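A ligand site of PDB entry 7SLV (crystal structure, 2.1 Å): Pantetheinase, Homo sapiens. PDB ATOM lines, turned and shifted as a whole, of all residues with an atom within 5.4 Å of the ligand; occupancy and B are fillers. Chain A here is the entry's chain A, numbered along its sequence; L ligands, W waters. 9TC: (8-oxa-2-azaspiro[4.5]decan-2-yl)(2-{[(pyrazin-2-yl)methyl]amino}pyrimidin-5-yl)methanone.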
ATOM      1  N   GLU A  78      36.194   7.048  21.134  1.00  0.00           N
ATOM      2  CA  GLU A  78      35.315   7.432  20.043  1.00  0.00           C
ATOM      3  C   GLU A  78      34.059   8.047  20.685  1.00  0.00           C
ATOM      4  O   GLU A  78      33.572   7.503  21.686  1.00  0.00           O
ATOM      5  CB  GLU A  78      34.894   6.187  19.271  1.00  0.00           C
ATOM      6  CG  GLU A  78      33.942   6.445  18.106  1.00  0.00           C
ATOM      7  CD  GLU A  78      33.398   5.199  17.465  1.00  0.00           C
ATOM      8  OE1 GLU A  78      33.454   4.136  18.122  1.00  0.00           O
ATOM      9  OE2 GLU A  78      32.935   5.269  16.304  1.00  0.00           O
ATOM     10  N   ASP A  79      33.527   9.160  20.108  1.00  0.00           N
ATOM     11  CA  ASP A  79      32.308   9.846  20.575  1.00  0.00           C
ATOM     12  C   ASP A  79      32.400  10.384  22.013  1.00  0.00           C
ATOM     13  O   ASP A  79      31.373  10.676  22.622  1.00  0.00           O
ATOM     14  CB  ASP A  79      31.078   8.893  20.478  1.00  0.00           C
ATOM     15  CG  ASP A  79      30.718   8.420  19.074  1.00  0.00           C
ATOM     16  OD1 ASP A  79      31.000   9.170  18.100  1.00  0.00           O
ATOM     17  OD2 ASP A  79      30.120   7.336  18.958  1.00  0.00           O
ATOM     18  N   TRP A  84      26.635   9.356  20.980  1.00  0.00           N
ATOM     19  CA  TRP A  84      26.266   8.606  19.782  1.00  0.00           C
ATOM     20  C   TRP A  84      24.774   8.646  19.392  1.00  0.00           C
ATOM     21  O   TRP A  84      24.361   7.869  18.526  1.00  0.00           O
ATOM     22  CB  TRP A  84      26.718   7.141  19.994  1.00  0.00           C
ATOM     23  CG  TRP A  84      26.273   6.597  21.319  1.00  0.00           C
ATOM     24  CD1 TRP A  84      25.035   6.117  21.642  1.00  0.00           C
ATOM     25  CD2 TRP A  84      27.034   6.587  22.537  1.00  0.00           C
ATOM     26  NE1 TRP A  84      24.977   5.798  22.986  1.00  0.00           N
ATOM     27  CE2 TRP A  84      26.195   6.080  23.557  1.00  0.00           C
ATOM     28  CE3 TRP A  84      28.341   6.988  22.882  1.00  0.00           C
ATOM     29  CZ2 TRP A  84      26.622   5.937  24.883  1.00  0.00           C
ATOM     30  CZ3 TRP A  84      28.761   6.856  24.196  1.00  0.00           C
ATOM     31  CH2 TRP A  84      27.922   6.326  25.178  1.00  0.00           C
ATOM     32  N   LYS A 177      36.209   7.399   9.690  1.00  0.00           N
ATOM     33  CA  LYS A 177      35.836   5.993   9.913  1.00  0.00           C
ATOM     34  C   LYS A 177      35.284   5.338   8.652  1.00  0.00           C
ATOM     35  O   LYS A 177      34.326   5.836   8.059  1.00  0.00           O
ATOM     36  CB  LYS A 177      34.856   5.856  11.089  1.00  0.00           C
ATOM     37  CG  LYS A 177      34.719   4.471  11.661  1.00  0.00           C
ATOM     38  CD  LYS A 177      33.701   4.482  12.831  1.00  0.00           C
ATOM     39  CE  LYS A 177      33.433   3.085  13.373  1.00  0.00           C
ATOM     40  NZ  LYS A 177      32.305   3.057  14.346  1.00  0.00           N
ATOM     41  N   PHE A 181      29.017   1.265  11.943  1.00  0.00           N
ATOM     42  CA  PHE A 181      28.207   0.294  12.677  1.00  0.00           C
ATOM     43  C   PHE A 181      26.715   0.583  12.475  1.00  0.00           C
ATOM     44  O   PHE A 181      26.370   1.643  11.977  1.00  0.00           O
ATOM     45  CB  PHE A 181      28.591   0.315  14.175  1.00  0.00           C
ATOM     46  CG  PHE A 181      28.069  -0.870  14.960  1.00  0.00           C
ATOM     47  CD1 PHE A 181      28.529  -2.162  14.692  1.00  0.00           C
ATOM     48  CD2 PHE A 181      27.150  -0.694  15.981  1.00  0.00           C
ATOM     49  CE1 PHE A 181      28.046  -3.256  15.422  1.00  0.00           C
ATOM     50  CE2 PHE A 181      26.664  -1.797  16.721  1.00  0.00           C
ATOM     51  CZ  PHE A 181      27.128  -3.070  16.442  1.00  0.00           C
ATOM     52  N   MET A 182      25.847  -0.390  12.831  1.00  0.00           N
ATOM     53  CA  MET A 182      24.389  -0.316  12.792  1.00  0.00           C
ATOM     54  C   MET A 182      23.868   0.994  13.416  1.00  0.00           C
ATOM     55  O   MET A 182      24.232   1.333  14.551  1.00  0.00           O
ATOM     56  CB  MET A 182      23.765  -1.518  13.551  1.00  0.00           C
ATOM     57  N   GLU A 184      24.504   4.200  12.361  1.00  0.00           N
ATOM     58  CA  GLU A 184      25.422   5.352  12.315  1.00  0.00           C
ATOM     59  C   GLU A 184      25.085   6.147  11.067  1.00  0.00           C
ATOM     60  O   GLU A 184      25.972   6.525  10.304  1.00  0.00           O
ATOM     61  CB  GLU A 184      26.888   4.933  12.356  1.00  0.00           C
ATOM     62  CG  GLU A 184      27.453   4.865  13.745  1.00  0.00           C
ATOM     63  CD  GLU A 184      28.964   4.695  13.816  1.00  0.00           C
ATOM     64  OE1 GLU A 184      29.500   3.794  13.136  1.00  0.00           O
ATOM     65  OE2 GLU A 184      29.595   5.451  14.590  1.00  0.00           O
ATOM     66  N   CYS A 210      37.046   1.836  16.476  1.00  0.00           N
ATOM     67  CA  CYS A 210      36.022   0.849  16.852  1.00  0.00           C
ATOM     68  C   CYS A 210      35.807  -0.316  15.846  1.00  0.00           C
ATOM     69  O   CYS A 210      36.667  -1.163  15.709  1.00  0.00           O
ATOM     70  CB  CYS A 210      34.704   1.576  17.136  1.00  0.00           C
ATOM     71  SG  CYS A 210      33.655   0.709  18.315  1.00  0.00           S
ATOM     72  N   PHE A 211      34.659  -0.334  15.155  1.00  0.00           N
ATOM     73  CA  PHE A 211      34.243  -1.381  14.213  1.00  0.00           C
ATOM     74  C   PHE A 211      35.256  -1.720  13.114  1.00  0.00           C
ATOM     75  O   PHE A 211      35.231  -2.825  12.580  1.00  0.00           O
ATOM     76  CB  PHE A 211      32.881  -1.014  13.601  1.00  0.00           C
ATOM     77  CG  PHE A 211      32.050  -2.157  13.049  1.00  0.00           C
ATOM     78  CD1 PHE A 211      31.938  -3.362  13.746  1.00  0.00           C
ATOM     79  CD2 PHE A 211      31.265  -1.983  11.915  1.00  0.00           C
ATOM     80  CE1 PHE A 211      31.107  -4.386  13.284  1.00  0.00           C
ATOM     81  CE2 PHE A 211      30.423  -3.005  11.461  1.00  0.00           C
ATOM     82  CZ  PHE A 211      30.334  -4.194  12.159  1.00  0.00           C
ATOM     83  N   LEU A 214      37.274  -5.082  12.866  1.00  0.00           N
ATOM     84  CA  LEU A 214      36.763  -6.328  12.298  1.00  0.00           C
ATOM     85  C   LEU A 214      36.902  -6.450  10.799  1.00  0.00           C
ATOM     86  O   LEU A 214      36.457  -7.451  10.244  1.00  0.00           O
ATOM     87  CB  LEU A 214      35.296  -6.522  12.707  1.00  0.00           C
ATOM     88  CG  LEU A 214      35.123  -7.114  14.088  1.00  0.00           C
ATOM     89  CD1 LEU A 214      33.691  -6.997  14.511  1.00  0.00           C
ATOM     90  CD2 LEU A 214      35.553  -8.582  14.097  1.00  0.00           C
ATOM     91  N   ALA A 236      34.036   2.964  21.075  1.00  0.00           N
ATOM     92  CA  ALA A 236      32.822   3.029  21.913  1.00  0.00           C
ATOM     93  C   ALA A 236      32.226   1.658  21.753  1.00  0.00           C
ATOM     94  O   ALA A 236      31.171   1.499  21.142  1.00  0.00           O
ATOM     95  CB  ALA A 236      31.873   4.124  21.426  1.00  0.00           C
ATOM     96  N   TRP A 237      32.944   0.651  22.254  1.00  0.00           N
ATOM     97  CA  TRP A 237      32.652  -0.777  22.103  1.00  0.00           C
ATOM     98  C   TRP A 237      31.617  -1.338  23.082  1.00  0.00           C
ATOM     99  O   TRP A 237      31.722  -1.125  24.289  1.00  0.00           O
ATOM    100  CB  TRP A 237      33.967  -1.564  22.206  1.00  0.00           C
ATOM    101  CG  TRP A 237      33.901  -2.985  21.709  1.00  0.00           C
ATOM    102  CD1 TRP A 237      33.558  -4.091  22.440  1.00  0.00           C
ATOM    103  CD2 TRP A 237      34.351  -3.463  20.438  1.00  0.00           C
ATOM    104  NE1 TRP A 237      33.760  -5.229  21.695  1.00  0.00           N
ATOM    105  CE2 TRP A 237      34.182  -4.869  20.435  1.00  0.00           C
ATOM    106  CE3 TRP A 237      34.817  -2.830  19.257  1.00  0.00           C
ATOM    107  CZ2 TRP A 237      34.511  -5.661  19.315  1.00  0.00           C
ATOM    108  CZ3 TRP A 237      35.134  -3.618  18.156  1.00  0.00           C
ATOM    109  CH2 TRP A 237      34.964  -5.011  18.182  1.00  0.00           C
ATOM    110  N   MET A 238      30.660  -2.084  22.554  1.00  0.00           N
ATOM    111  CA  MET A 238      29.631  -2.794  23.327  1.00  0.00           C
ATOM    112  C   MET A 238      30.073  -4.245  23.445  1.00  0.00           C
ATOM    113  O   MET A 238      30.141  -4.946  22.438  1.00  0.00           O
ATOM    114  CB  MET A 238      28.257  -2.661  22.685  1.00  0.00           C
ATOM    115  CG  MET A 238      27.734  -1.245  22.735  1.00  0.00           C
ATOM    116  SD  MET A 238      26.112  -1.012  21.964  1.00  0.00           S
ATOM    117  CE  MET A 238      26.455  -1.434  20.297  1.00  0.00           C
ATOM    118  N   ASN A 239      30.441  -4.651  24.660  1.00  0.00           N
ATOM    119  CA  ASN A 239      30.932  -5.992  24.983  1.00  0.00           C
ATOM    120  C   ASN A 239      29.946  -7.094  24.637  1.00  0.00           C
ATOM    121  O   ASN A 239      28.761  -7.003  24.971  1.00  0.00           O
ATOM    122  CB  ASN A 239      31.346  -6.059  26.462  1.00  0.00           C
ATOM    123  CG  ASN A 239      32.514  -5.168  26.801  1.00  0.00           C
ATOM    124  OD1 ASN A 239      33.412  -4.900  25.959  1.00  0.00           O
ATOM    125  ND2 ASN A 239      32.549  -4.717  28.051  1.00  0.00           N
ATOM    126  N   VAL A 240      30.412  -8.101  23.880  1.00  0.00           N
ATOM    127  CA  VAL A 240      29.602  -9.275  23.494  1.00  0.00           C
ATOM    128  C   VAL A 240      30.413 -10.525  23.793  1.00  0.00           C
ATOM    129  O   VAL A 240      31.261 -10.905  22.997  1.00  0.00           O
ATOM    130  CB  VAL A 240      29.068  -9.259  22.021  1.00  0.00           C
ATOM    131  CG1 VAL A 240      28.352 -10.575  21.696  1.00  0.00           C
ATOM    132  CG2 VAL A 240      28.139  -8.088  21.770  1.00  0.00           C
ATOM    133  N   LEU A 244      33.699 -11.284  21.911  1.00  0.00           N
ATOM    134  CA  LEU A 244      33.839  -9.895  21.530  1.00  0.00           C
ATOM    135  C   LEU A 244      33.749  -8.914  22.681  1.00  0.00           C
ATOM    136  O   LEU A 244      33.138  -7.854  22.556  1.00  0.00           O
ATOM    137  CB  LEU A 244      32.862  -9.591  20.380  1.00  0.00           C
ATOM    138  CG  LEU A 244      33.239 -10.327  19.047  1.00  0.00           C
ATOM    139  CD1 LEU A 244      32.209 -10.108  18.000  1.00  0.00           C
ATOM    140  CD2 LEU A 244      34.625  -9.878  18.497  1.00  0.00           C
ATOM    141  N   LYS A 271      25.231   0.145  28.658  1.00  0.00           N
ATOM    142  CA  LYS A 271      25.272  -0.300  27.252  1.00  0.00           C
ATOM    143  C   LYS A 271      26.383  -1.332  27.071  1.00  0.00           C
ATOM    144  O   LYS A 271      26.716  -1.689  25.941  1.00  0.00           O
ATOM    145  CB  LYS A 271      25.464   0.870  26.282  1.00  0.00           C
ATOM    146  CG  LYS A 271      24.170   1.526  25.850  1.00  0.00           C
ATOM    147  CD  LYS A 271      24.365   2.574  24.750  1.00  0.00           C
ATOM    148  CE  LYS A 271      24.377   2.001  23.343  1.00  0.00           C
ATOM    149  NZ  LYS A 271      23.062   1.443  22.932  1.00  0.00           N
ATOM    150  N   MET A 273      29.578  -0.924  27.883  1.00  0.00           N
ATOM    151  CA  MET A 273      30.778  -0.259  27.390  1.00  0.00           C
ATOM    152  C   MET A 273      31.765  -0.098  28.528  1.00  0.00           C
ATOM    153  O   MET A 273      31.511   0.629  29.499  1.00  0.00           O
ATOM    154  CB  MET A 273      30.452   1.099  26.725  1.00  0.00           C
ATOM    155  CG  MET A 273      29.394   1.012  25.604  1.00  0.00           C
ATOM    156  SD  MET A 273      28.987   2.671  24.995  1.00  0.00           S
ATOM    157  CE  MET A 273      28.494   2.309  23.450  1.00  0.00           C
ATOM    158  N   PHE A 337      26.668 -15.831  19.859  1.00  0.00           N
ATOM    159  CA  PHE A 337      26.443 -14.527  19.227  1.00  0.00           C
ATOM    160  C   PHE A 337      25.682 -14.670  17.872  1.00  0.00           C
ATOM    161  O   PHE A 337      26.150 -14.220  16.809  1.00  0.00           O
ATOM    162  CB  PHE A 337      27.770 -13.728  19.124  1.00  0.00           C
ATOM    163  CG  PHE A 337      27.663 -12.312  18.601  1.00  0.00           C
ATOM    164  CD1 PHE A 337      26.536 -11.534  18.875  1.00  0.00           C
ATOM    165  CD2 PHE A 337      28.698 -11.741  17.872  1.00  0.00           C
ATOM    166  CE1 PHE A 337      26.440 -10.228  18.394  1.00  0.00           C
ATOM    167  CE2 PHE A 337      28.602 -10.434  17.391  1.00  0.00           C
ATOM    168  CZ  PHE A 337      27.472  -9.688  17.647  1.00  0.00           C
ATOM    169  N   HIS A 386      28.831 -14.225   9.632  1.00  0.00           N
ATOM    170  CA  HIS A 386      28.069 -13.572  10.712  1.00  0.00           C
ATOM    171  C   HIS A 386      27.204 -12.518  10.013  1.00  0.00           C
ATOM    172  O   HIS A 386      27.692 -11.834   9.121  1.00  0.00           O
ATOM    173  CB  HIS A 386      28.987 -12.911  11.748  1.00  0.00           C
ATOM    174  CG  HIS A 386      28.245 -12.297  12.883  1.00  0.00           C
ATOM    175  ND1 HIS A 386      28.058 -12.974  14.060  1.00  0.00           N
ATOM    176  CD2 HIS A 386      27.625 -11.096  12.965  1.00  0.00           C
ATOM    177  CE1 HIS A 386      27.336 -12.181  14.817  1.00  0.00           C
ATOM    178  NE2 HIS A 386      27.054 -11.038  14.205  1.00  0.00           N
ATOM    179  N   VAL A 388      24.213 -10.836  11.954  1.00  0.00           N
ATOM    180  CA  VAL A 388      23.495 -10.014  12.940  1.00  0.00           C
ATOM    181  C   VAL A 388      24.342  -8.808  13.427  1.00  0.00           C
ATOM    182  O   VAL A 388      25.338  -8.977  14.144  1.00  0.00           O
ATOM    183  CB  VAL A 388      22.929 -10.846  14.112  1.00  0.00           C
ATOM    184  CG1 VAL A 388      22.256  -9.955  15.166  1.00  0.00           C
ATOM    185  CG2 VAL A 388      21.944 -11.911  13.602  1.00  0.00           C
ATOM    186  N   GLU A 389      23.896  -7.588  13.078  1.00  0.00           N
ATOM    187  CA  GLU A 389      24.525  -6.299  13.409  1.00  0.00           C
ATOM    188  C   GLU A 389      25.924  -6.165  12.759  1.00  0.00           C
ATOM    189  O   GLU A 389      26.820  -5.528  13.333  1.00  0.00           O
ATOM    190  CB  GLU A 389      24.574  -6.061  14.942  1.00  0.00           C
ATOM    191  CG  GLU A 389      23.236  -5.837  15.624  1.00  0.00           C
ATOM    192  CD  GLU A 389      23.240  -6.050  17.135  1.00  0.00           C
ATOM    193  OE1 GLU A 389      24.199  -5.608  17.812  1.00  0.00           O
ATOM    194  OE2 GLU A 389      22.262  -6.648  17.639  1.00  0.00           O
ATOM    195  N   GLY A 390      26.101  -6.726  11.566  1.00  0.00           N
ATOM    196  CA  GLY A 390      27.362  -6.677  10.842  1.00  0.00           C
ATOM    197  C   GLY A 390      27.588  -7.943  10.071  1.00  0.00           C
ATOM    198  O   GLY A 390      27.271  -9.022  10.560  1.00  0.00           O
ATOM    199  N   TYR A 392      30.298 -10.320   8.284  1.00  0.00           N
ATOM    200  CA  TYR A 392      31.713 -10.669   8.224  1.00  0.00           C
ATOM    201  C   TYR A 392      31.899 -12.141   8.335  1.00  0.00           C
ATOM    202  O   TYR A 392      31.240 -12.793   9.161  1.00  0.00           O
ATOM    203  CB  TYR A 392      32.555  -9.892   9.284  1.00  0.00           C
ATOM    204  CG  TYR A 392      31.956  -9.798  10.670  1.00  0.00           C
ATOM    205  CD1 TYR A 392      32.212 -10.766  11.625  1.00  0.00           C
ATOM    206  CD2 TYR A 392      31.247  -8.659  11.073  1.00  0.00           C
ATOM    207  CE1 TYR A 392      31.694 -10.673  12.906  1.00  0.00           C
ATOM    208  CE2 TYR A 392      30.698  -8.571  12.352  1.00  0.00           C
ATOM    209  CZ  TYR A 392      30.931  -9.579  13.270  1.00  0.00           C
ATOM    210  OH  TYR A 392      30.463  -9.483  14.555  1.00  0.00           O
HETATM  211  N3  9TC L   1      30.748  -4.641  19.606  1.00  0.00           N
HETATM  212  C4  9TC L   1      30.346  -6.673  16.551  1.00  0.00           C
HETATM  213  N2  9TC L   1      29.411  -7.027  15.645  1.00  0.00           N
HETATM  214  C7  9TC L   1      30.377  -1.134  19.181  1.00  0.00           C
HETATM  215  C6  9TC L   1      30.694  -3.414  18.984  1.00  0.00           C
HETATM  216  C9  9TC L   1      31.039  -2.107  17.106  1.00  0.00           C
HETATM  217  C13 9TC L   1      28.344   2.869  18.532  1.00  0.00           C
HETATM  218  C8  9TC L   1      30.680  -0.945  17.837  1.00  0.00           C
HETATM  219  N5  9TC L   1      31.052  -3.335  17.634  1.00  0.00           N
HETATM  220  C18 9TC L   1      27.976   3.413  19.903  1.00  0.00           C
HETATM  221  C16 9TC L   1      25.937   2.145  18.353  1.00  0.00           C
HETATM  222  C1  9TC L   1      28.130  -6.887  16.017  1.00  0.00           C
HETATM  223  C2  9TC L   1      27.771  -6.402  17.295  1.00  0.00           C
HETATM  224  N1  9TC L   1      28.702  -6.067  18.221  1.00  0.00           N
HETATM  225  C3  9TC L   1      29.996  -6.199  17.840  1.00  0.00           C
HETATM  226  C5  9TC L   1      31.065  -5.839  18.845  1.00  0.00           C
HETATM  227  N4  9TC L   1      30.347  -2.330  19.783  1.00  0.00           N
HETATM  228  C10 9TC L   1      30.742   0.339  17.138  1.00  0.00           C
HETATM  229  O1  9TC L   1      31.425   0.485  16.119  1.00  0.00           O
HETATM  230  N6  9TC L   1      30.080   1.449  17.649  1.00  0.00           N
HETATM  231  C11 9TC L   1      30.225   2.763  16.984  1.00  0.00           C
HETATM  232  C12 9TC L   1      29.445   3.730  17.881  1.00  0.00           C
HETATM  233  C14 9TC L   1      28.967   1.447  18.611  1.00  0.00           C
HETATM  234  C15 9TC L   1      27.093   2.861  17.650  1.00  0.00           C
HETATM  235  O2  9TC L   1      25.677   2.724  19.609  1.00  0.00           O
HETATM  236  C17 9TC L   1      26.774   2.653  20.486  1.00  0.00           C
HETATM  237  O   HOH W   1      26.682  -5.256  20.448  1.00  0.00           O
HETATM  238  O   HOH W   2      28.776   6.863  16.652  1.00  0.00           O
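N4 of the ligand lies within hydrogen-bond range of N of Met 238 (2.8 Å). O of Met 238 is in hydrogen-bond range of N3 of the ligand, at 2.9 Å. The side-chain hydroxyl (OH) of Tyr 392 sits at hydrogen-bond distance from a nitrogen (N2) of the ligand (2.9 Å). An oxygen (O1) of the ligand lies within hydrogen-bond range of the side-chain sulfur (SG) of Cys 210 (3.1 Å). O1 of the ligand lies within hydrogen-bond range of NZ of Lys 177, at 3.2 Å. The backbone NH (N) of Phe 211 sits close to an oxygen (O1) of the ligand (3.5 Å).
N of His 386 is in hydrogen-bond range of O of Tyr 392, 2.8 Å away. The side-chain sulfur (SG) of Cys 210 sits at hydrogen-bond distance from the backbone NH (N) of Ala 236, 3.6 Å away. SG of Cys 210 lies close to OE1 of Glu 78 (3.4 Å). The side-chain amino group of Lys 177 is in salt-bridge range of the side-chain carboxylate of Glu 184 (3.1 Å). N of Ala 236 sits at hydrogen-bond distance from OE1 of Glu 78 (3.2 Å). The backbone NH (N) of Phe 181 sits at hydrogen-bond distance from the side-chain carboxylate (OE1) of Glu 184. NE1 of Trp 237 lies within hydrogen-bond range of O of Leu 244, at 2.8 Å. The backbone carbonyl oxygen (O) of Val 388 sits at hydrogen-bond distance from a ring nitrogen (NE2) of His 386 (2.7 Å).
Residues that only touch the ligand: Glu 78 (3.7 Å), Asp 79 (3.8 Å), Trp 84 (3.9 Å), Phe 181 (3.4 Å), Glu 184 (3.7 Å), Leu 214 (3.9 Å), Ala 236 (3.4 Å), Trp 237 (3.5 Å), Lys 271 (3.8 Å), Met 273 (3.4 Å), Phe 337 (3.3 Å), Val 388 (3.96 Å) and Glu 389 (3.3 Å). Hydrophobic or aromatic side chains within 4 Å of the ligand: Trp 84, Phe 181, Phe 211, Leu 214, Trp 237, Met 238, Met 273, Phe 337 and Tyr 392. Within 4 Å of the ligand: Glu 78, Asp 79, Trp 84, Lys 177, Phe 181, Glu 184, Cys 210, Phe 211, Leu 214, Ala 236, Trp 237, Met 238, Lys 271, Met 273, Phe 337, Val 388, Glu 389 and Tyr 392. The nearest printed residue that does not touch the ligand is Val 240 (4.1 Å).
Water W2 bridges OE2 of Glu 184 (2.6 Å) and OD2 of Asp 79 (2.7 Å).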
